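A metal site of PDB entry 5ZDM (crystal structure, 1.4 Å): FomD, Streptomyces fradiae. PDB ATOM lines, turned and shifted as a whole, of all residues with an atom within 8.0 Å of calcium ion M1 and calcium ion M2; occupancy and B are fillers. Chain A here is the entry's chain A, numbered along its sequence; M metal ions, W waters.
Calcium ion M2 is bound by OD1 of Asn 113 (2.2 Å), OD1 of Asp 129 (2.4 Å), OD1 of Asp 133 (2.4 Å), water W1 (2.4 Å) and water W2 (2.4 Å).
Calcium ion M1 is bound by the backbone carbonyl oxygen (O) of Glu 131 (2.3 Å).
The side-chain carboxylate (OE1) of Glu 131 is bound to calcium ion M1 (2.3 Å).
OD2 of Asp 147 binds calcium ion M1, at 2.4 Å.
Calcium ion M1 is bound by OD2 of Asp 133, at 2.4 Å.
Water W2 is bound to calcium ion M1 (2.5 Å).
Calcium ion M1 is bound by the side-chain carboxylate (OD1) of Asp 133.
Water W1 lies within hydrogen-bond range of O of Ile 132, O of Val 114 and N of Glu 131.
Within 4 Å of calcium ion M2: Asn 113, Asp 129 and Asp 133.
Along chain A the residues within 4 Å of calcium ion M2 span positions 113 to 133.
ND2 of Asn 113 is in hydrogen-bond range of OE1 of Glu 115 (2.8 Å).
The side-chain carboxylate (OD2) of Asp 129 sits at hydrogen-bond distance from the backbone NH (N) of Glu 131 (2.9 Å).
The side-chain amino group of Lys 150 is in salt-bridge range of the side-chain carboxylate of Glu 131, 3.0 Å away.
The side-chain carboxylate (OE2) of Glu 131 lies within salt-bridge range of the guanidinium group (NH1) of Arg 154, 2.8 Å away.
The side-chain carboxylate (OD1) of Asp 147 is in salt-bridge range of the side-chain amino group (NZ) of Lys 146, 3.98 Å away.
The backbone carbonyl oxygen (O) of Asp 133 lies within hydrogen-bond range of the backbone NH (N) of Lys 146 (2.8 Å).
N of Asp 129 lies within hydrogen-bond range of OD2 of Asp 26, at 2.9 Å.
NZ of Lys 146 lies within hydrogen-bond range of OH of Tyr 111 (3.0 Å).
Residues that only touch calcium ion M1: Lys 146 (3.9 Å).
Within 4 Å of calcium ion M1: Glu 131, Asp 133, Lys 146 and Asp 147.
The nearest printed residue that does not touch calcium ion M1 is Ile 132 (4.5 Å).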
ATOM      1  N   ASP A  26      15.889 -16.630  -2.281  1.00  0.00           N
ATOM      2  CA  ASP A  26      16.819 -17.281  -1.392  1.00  0.00           C
ATOM      3  C   ASP A  26      16.459 -16.871   0.041  1.00  0.00           C
ATOM      4  O   ASP A  26      16.395 -15.641   0.298  1.00  0.00           O
ATOM      5  CB  ASP A  26      18.331 -16.924  -1.594  1.00  0.00           C
ATOM      6  CG  ASP A  26      18.915 -17.472  -2.819  1.00  0.00           C
ATOM      7  OD1 ASP A  26      18.498 -17.100  -3.914  1.00  0.00           O
ATOM      8  OD2 ASP A  26      19.818 -18.296  -2.706  1.00  0.00           O
ATOM      9  N   TRP A  97      21.694 -23.175 -14.570  1.00  0.00           N
ATOM     10  CA  TRP A  97      21.453 -21.872 -15.202  1.00  0.00           C
ATOM     11  C   TRP A  97      22.066 -21.886 -16.593  1.00  0.00           C
ATOM     12  O   TRP A  97      23.216 -22.324 -16.795  1.00  0.00           O
ATOM     13  CB  TRP A  97      22.100 -20.784 -14.387  1.00  0.00           C
ATOM     14  CG  TRP A  97      21.577 -20.638 -13.012  1.00  0.00           C
ATOM     15  CD1 TRP A  97      20.665 -21.417 -12.351  1.00  0.00           C
ATOM     16  CD2 TRP A  97      21.991 -19.638 -12.058  1.00  0.00           C
ATOM     17  NE1 TRP A  97      20.471 -20.971 -11.053  1.00  0.00           N
ATOM     18  CE2 TRP A  97      21.238 -19.835 -10.870  1.00  0.00           C
ATOM     19  CE3 TRP A  97      22.931 -18.615 -12.101  1.00  0.00           C
ATOM     20  CZ2 TRP A  97      21.445 -19.087  -9.736  1.00  0.00           C
ATOM     21  CZ3 TRP A  97      23.111 -17.838 -11.003  1.00  0.00           C
ATOM     22  CH2 TRP A  97      22.321 -18.052  -9.832  1.00  0.00           C
ATOM     23  N   TYR A 111      25.631 -23.468 -15.818  1.00  0.00           N
ATOM     24  CA  TYR A 111      26.146 -23.129 -14.457  1.00  0.00           C
ATOM     25  C   TYR A 111      25.297 -23.851 -13.427  1.00  0.00           C
ATOM     26  O   TYR A 111      24.145 -23.554 -13.262  1.00  0.00           O
ATOM     27  CB  TYR A 111      26.199 -21.666 -14.316  1.00  0.00           C
ATOM     28  CG  TYR A 111      26.879 -21.153 -13.062  1.00  0.00           C
ATOM     29  CD1 TYR A 111      28.197 -20.939 -13.073  1.00  0.00           C
ATOM     30  CD2 TYR A 111      26.159 -20.922 -11.895  1.00  0.00           C
ATOM     31  CE1 TYR A 111      28.827 -20.483 -11.917  1.00  0.00           C
ATOM     32  CE2 TYR A 111      26.780 -20.409 -10.757  1.00  0.00           C
ATOM     33  CZ  TYR A 111      28.125 -20.228 -10.773  1.00  0.00           C
ATOM     34  OH  TYR A 111      28.837 -19.702  -9.687  1.00  0.00           O
ATOM     35  N   VAL A 112      25.874 -24.873 -12.835  1.00  0.00           N
ATOM     36  CA  VAL A 112      25.169 -25.706 -11.849  1.00  0.00           C
ATOM     37  C   VAL A 112      25.279 -24.987 -10.470  1.00  0.00           C
ATOM     38  O   VAL A 112      26.369 -24.890  -9.925  1.00  0.00           O
ATOM     39  CB  VAL A 112      25.710 -27.102 -11.738  1.00  0.00           C
ATOM     40  CG1 VAL A 112      24.899 -27.898 -10.737  1.00  0.00           C
ATOM     41  CG2 VAL A 112      25.686 -27.762 -13.130  1.00  0.00           C
ATOM     42  N   ASN A 113      24.161 -24.469  -9.987  1.00  0.00           N
ATOM     43  CA  ASN A 113      24.112 -23.786  -8.737  1.00  0.00           C
ATOM     44  C   ASN A 113      23.579 -24.713  -7.688  1.00  0.00           C
ATOM     45  O   ASN A 113      22.390 -24.974  -7.598  1.00  0.00           O
ATOM     46  CB  ASN A 113      23.184 -22.538  -8.942  1.00  0.00           C
ATOM     47  CG  ASN A 113      23.568 -21.468  -7.884  1.00  0.00           C
ATOM     48  OD1 ASN A 113      24.717 -21.024  -7.908  1.00  0.00           O
ATOM     49  ND2 ASN A 113      22.636 -21.237  -6.866  1.00  0.00           N
ATOM     50  N   VAL A 114      24.479 -25.242  -6.845  1.00  0.00           N
ATOM     51  CA  VAL A 114      24.080 -26.139  -5.767  1.00  0.00           C
ATOM     52  C   VAL A 114      23.400 -25.280  -4.715  1.00  0.00           C
ATOM     53  O   VAL A 114      23.886 -24.170  -4.401  1.00  0.00           O
ATOM     54  CB  VAL A 114      25.345 -26.851  -5.222  1.00  0.00           C
ATOM     55  CG1 VAL A 114      24.982 -27.830  -4.135  1.00  0.00           C
ATOM     56  CG2 VAL A 114      26.030 -27.600  -6.381  1.00  0.00           C
ATOM     57  N   GLU A 115      22.267 -25.706  -4.285  1.00  0.00           N
ATOM     58  CA  GLU A 115      21.321 -24.905  -3.457  1.00  0.00           C
ATOM     59  C   GLU A 115      20.254 -25.802  -2.919  1.00  0.00           C
ATOM     60  O   GLU A 115      20.063 -26.983  -3.398  1.00  0.00           O
ATOM     61  CB  GLU A 115      20.736 -23.770  -4.296  1.00  0.00           C
ATOM     62  CG  GLU A 115      19.874 -24.253  -5.499  1.00  0.00           C
ATOM     63  CD  GLU A 115      19.492 -23.155  -6.381  1.00  0.00           C
ATOM     64  OE1 GLU A 115      20.006 -22.028  -6.344  1.00  0.00           O
ATOM     65  OE2 GLU A 115      18.675 -23.466  -7.340  1.00  0.00           O
ATOM     66  N   LEU A 128      18.056 -21.710  -1.283  1.00  0.00           N
ATOM     67  CA  LEU A 128      19.182 -21.045  -0.634  1.00  0.00           C
ATOM     68  C   LEU A 128      20.490 -21.512  -1.242  1.00  0.00           C
ATOM     69  O   LEU A 128      20.704 -22.706  -1.278  1.00  0.00           O
ATOM     70  CB  LEU A 128      19.214 -21.196   0.925  1.00  0.00           C
ATOM     71  CG  LEU A 128      20.362 -20.548   1.585  1.00  0.00           C
ATOM     72  CD1 LEU A 128      20.367 -19.028   1.379  1.00  0.00           C
ATOM     73  CD2 LEU A 128      20.361 -20.902   3.084  1.00  0.00           C
ATOM     74  N   ASP A 129      21.305 -20.611  -1.712  1.00  0.00           N
ATOM     75  CA  ASP A 129      22.597 -20.961  -2.347  1.00  0.00           C
ATOM     76  C   ASP A 129      23.434 -21.779  -1.394  1.00  0.00           C
ATOM     77  O   ASP A 129      23.543 -21.428  -0.178  1.00  0.00           O
ATOM     78  CB  ASP A 129      23.319 -19.719  -2.727  1.00  0.00           C
ATOM     79  CG  ASP A 129      24.572 -19.961  -3.477  1.00  0.00           C
ATOM     80  OD1 ASP A 129      24.474 -20.172  -4.746  1.00  0.00           O
ATOM     81  OD2 ASP A 129      25.684 -20.023  -2.871  1.00  0.00           O
ATOM     82  N   HIS A 130      24.083 -22.842  -1.860  1.00  0.00           N
ATOM     83  CA  HIS A 130      24.943 -23.744  -1.080  1.00  0.00           C
ATOM     84  C   HIS A 130      26.409 -23.695  -1.489  1.00  0.00           C
ATOM     85  O   HIS A 130      27.164 -24.631  -1.218  1.00  0.00           O
ATOM     86  CB  HIS A 130      24.402 -25.148  -1.087  1.00  0.00           C
ATOM     87  CG  HIS A 130      23.139 -25.338  -0.300  1.00  0.00           C
ATOM     88  ND1 HIS A 130      22.356 -26.489  -0.374  1.00  0.00           N
ATOM     89  CD2 HIS A 130      22.550 -24.527   0.591  1.00  0.00           C
ATOM     90  CE1 HIS A 130      21.394 -26.358   0.512  1.00  0.00           C
ATOM     91  NE2 HIS A 130      21.470 -25.181   1.067  1.00  0.00           N
ATOM     92  N   GLU A 131      26.826 -22.573  -2.061  1.00  0.00           N
ATOM     93  CA  GLU A 131      28.187 -22.166  -2.393  1.00  0.00           C
ATOM     94  C   GLU A 131      28.846 -22.994  -3.505  1.00  0.00           C
ATOM     95  O   GLU A 131      29.367 -22.404  -4.431  1.00  0.00           O
ATOM     96  CB  GLU A 131      29.098 -22.098  -1.131  1.00  0.00           C
ATOM     97  CG  GLU A 131      30.450 -21.535  -1.473  1.00  0.00           C
ATOM     98  CD  GLU A 131      30.365 -20.147  -1.959  1.00  0.00           C
ATOM     99  OE1 GLU A 131      30.519 -19.883  -3.171  1.00  0.00           O
ATOM    100  OE2 GLU A 131      30.123 -19.263  -1.068  1.00  0.00           O
ATOM    101  N   ILE A 132      28.924 -24.293  -3.423  1.00  0.00           N
ATOM    102  CA  ILE A 132      29.580 -25.077  -4.474  1.00  0.00           C
ATOM    103  C   ILE A 132      28.839 -24.809  -5.804  1.00  0.00           C
ATOM    104  O   ILE A 132      27.633 -24.759  -5.853  1.00  0.00           O
ATOM    105  CB  ILE A 132      29.578 -26.603  -4.167  1.00  0.00           C
ATOM    106  CG1 ILE A 132      30.264 -26.872  -2.810  1.00  0.00           C
ATOM    107  CG2 ILE A 132      30.260 -27.374  -5.328  1.00  0.00           C
ATOM    108  CD1 ILE A 132      30.407 -28.322  -2.527  1.00  0.00           C
ATOM    109  N   ASP A 133      29.590 -24.630  -6.864  1.00  0.00           N
ATOM    110  CA  ASP A 133      29.013 -24.503  -8.232  1.00  0.00           C
ATOM    111  C   ASP A 133      29.812 -25.408  -9.114  1.00  0.00           C
ATOM    112  O   ASP A 133      30.915 -25.833  -8.836  1.00  0.00           O
ATOM    113  CB  ASP A 133      29.091 -23.092  -8.738  1.00  0.00           C
ATOM    114  CG  ASP A 133      29.139 -22.026  -7.696  1.00  0.00           C
ATOM    115  OD1 ASP A 133      28.102 -21.625  -7.183  1.00  0.00           O
ATOM    116  OD2 ASP A 133      30.254 -21.605  -7.341  1.00  0.00           O
ATOM    117  N   LEU A 134      29.202 -25.833 -10.243  1.00  0.00           N
ATOM    118  CA  LEU A 134      29.909 -26.571 -11.313  1.00  0.00           C
ATOM    119  C   LEU A 134      29.663 -25.844 -12.604  1.00  0.00           C
ATOM    120  O   LEU A 134      28.610 -25.255 -12.779  1.00  0.00           O
ATOM    121  CB  LEU A 134      29.532 -28.003 -11.398  1.00  0.00           C
ATOM    122  CG  LEU A 134      29.408 -28.912 -10.204  1.00  0.00           C
ATOM    123  CD1 LEU A 134      28.829 -30.242 -10.775  1.00  0.00           C
ATOM    124  CD2 LEU A 134      30.694 -29.037  -9.623  1.00  0.00           C
ATOM    125  N   LYS A 146      33.740 -25.569  -8.784  1.00  0.00           N
ATOM    126  CA  LYS A 146      33.981 -24.176  -8.395  1.00  0.00           C
ATOM    127  C   LYS A 146      33.647 -23.922  -6.924  1.00  0.00           C
ATOM    128  O   LYS A 146      32.635 -24.422  -6.434  1.00  0.00           O
ATOM    129  CB  LYS A 146      33.131 -23.345  -9.316  1.00  0.00           C
ATOM    130  CG  LYS A 146      33.269 -21.846  -9.134  1.00  0.00           C
ATOM    131  CD  LYS A 146      32.494 -21.045 -10.164  1.00  0.00           C
ATOM    132  CE  LYS A 146      32.373 -19.608  -9.922  1.00  0.00           C
ATOM    133  NZ  LYS A 146      31.618 -19.276  -8.682  1.00  0.00           N
ATOM    134  N   ASP A 147      34.487 -23.219  -6.232  1.00  0.00           N
ATOM    135  CA  ASP A 147      34.243 -22.739  -4.900  1.00  0.00           C
ATOM    136  C   ASP A 147      34.172 -23.807  -3.851  1.00  0.00           C
ATOM    137  O   ASP A 147      33.544 -23.609  -2.806  1.00  0.00           O
ATOM    138  CB  ASP A 147      32.974 -21.894  -4.867  1.00  0.00           C
ATOM    139  CG  ASP A 147      33.138 -20.503  -5.521  1.00  0.00           C
ATOM    140  OD1 ASP A 147      34.306 -20.065  -5.855  1.00  0.00           O
ATOM    141  OD2 ASP A 147      32.149 -19.828  -5.810  1.00  0.00           O
ATOM    142  N   VAL A 148      34.827 -24.957  -4.089  1.00  0.00           N
ATOM    143  CA  VAL A 148      34.834 -26.013  -3.065  1.00  0.00           C
ATOM    144  C   VAL A 148      35.557 -25.564  -1.779  1.00  0.00           C
ATOM    145  O   VAL A 148      35.027 -25.720  -0.711  1.00  0.00           O
ATOM    146  CB  VAL A 148      35.403 -27.327  -3.551  1.00  0.00           C
ATOM    147  CG1 VAL A 148      35.506 -28.362  -2.440  1.00  0.00           C
ATOM    148  CG2 VAL A 148      34.443 -27.880  -4.625  1.00  0.00           C
ATOM    149  N   LYS A 150      36.160 -22.527  -0.806  1.00  0.00           N
ATOM    150  CA  LYS A 150      35.374 -21.428  -0.239  1.00  0.00           C
ATOM    151  C   LYS A 150      34.224 -21.994   0.598  1.00  0.00           C
ATOM    152  O   LYS A 150      34.017 -21.569   1.720  1.00  0.00           O
ATOM    153  CB  LYS A 150      34.866 -20.540  -1.351  1.00  0.00           C
ATOM    154  CG  LYS A 150      34.094 -19.369  -0.879  1.00  0.00           C
ATOM    155  CD  LYS A 150      33.545 -18.679  -2.128  1.00  0.00           C
ATOM    156  CE  LYS A 150      32.700 -17.545  -1.645  1.00  0.00           C
ATOM    157  NZ  LYS A 150      31.687 -17.243  -2.617  1.00  0.00           N
ATOM    158  N   PHE A 151      33.526 -22.977   0.044  1.00  0.00           N
ATOM    159  CA  PHE A 151      32.481 -23.689   0.773  1.00  0.00           C
ATOM    160  C   PHE A 151      33.036 -24.297   2.101  1.00  0.00           C
ATOM    161  O   PHE A 151      32.422 -24.155   3.140  1.00  0.00           O
ATOM    162  CB  PHE A 151      31.849 -24.752  -0.121  1.00  0.00           C
ATOM    163  CG  PHE A 151      31.052 -25.754   0.632  1.00  0.00           C
ATOM    164  CD1 PHE A 151      29.849 -25.418   1.171  1.00  0.00           C
ATOM    165  CD2 PHE A 151      31.594 -27.000   0.865  1.00  0.00           C
ATOM    166  CE1 PHE A 151      29.113 -26.351   1.937  1.00  0.00           C
ATOM    167  CE2 PHE A 151      30.849 -27.937   1.592  1.00  0.00           C
ATOM    168  CZ  PHE A 151      29.648 -27.593   2.094  1.00  0.00           C
ATOM    169  N   ARG A 154      33.605 -21.708   4.724  1.00  0.00           N
ATOM    170  CA  ARG A 154      32.375 -21.362   5.321  1.00  0.00           C
ATOM    171  C   ARG A 154      31.734 -22.420   6.184  1.00  0.00           C
ATOM    172  O   ARG A 154      31.139 -22.044   7.254  1.00  0.00           O
ATOM    173  CB  ARG A 154      31.406 -20.910   4.174  1.00  0.00           C
ATOM    174  CG  ARG A 154      31.865 -19.667   3.470  1.00  0.00           C
ATOM    175  CD  ARG A 154      30.900 -19.161   2.325  1.00  0.00           C
ATOM    176  NE  ARG A 154      29.625 -18.887   2.927  1.00  0.00           N
ATOM    177  CZ  ARG A 154      28.442 -18.996   2.347  1.00  0.00           C
ATOM    178  NH1 ARG A 154      28.367 -19.334   1.051  1.00  0.00           N
ATOM    179  NH2 ARG A 154      27.363 -18.760   3.051  1.00  0.00           N
HETATM  180 CA    CA M   1      29.888 -20.366  -5.348  1.00  0.00          CA
HETATM  181 CA    CA M   2      26.194 -20.454  -6.367  1.00  0.00          CA
HETATM  182  O   HOH W   1      26.013 -22.622  -5.364  1.00  0.00           O
HETATM  183  O   HOH W   2      27.617 -19.489  -4.645  1.00  0.00           O
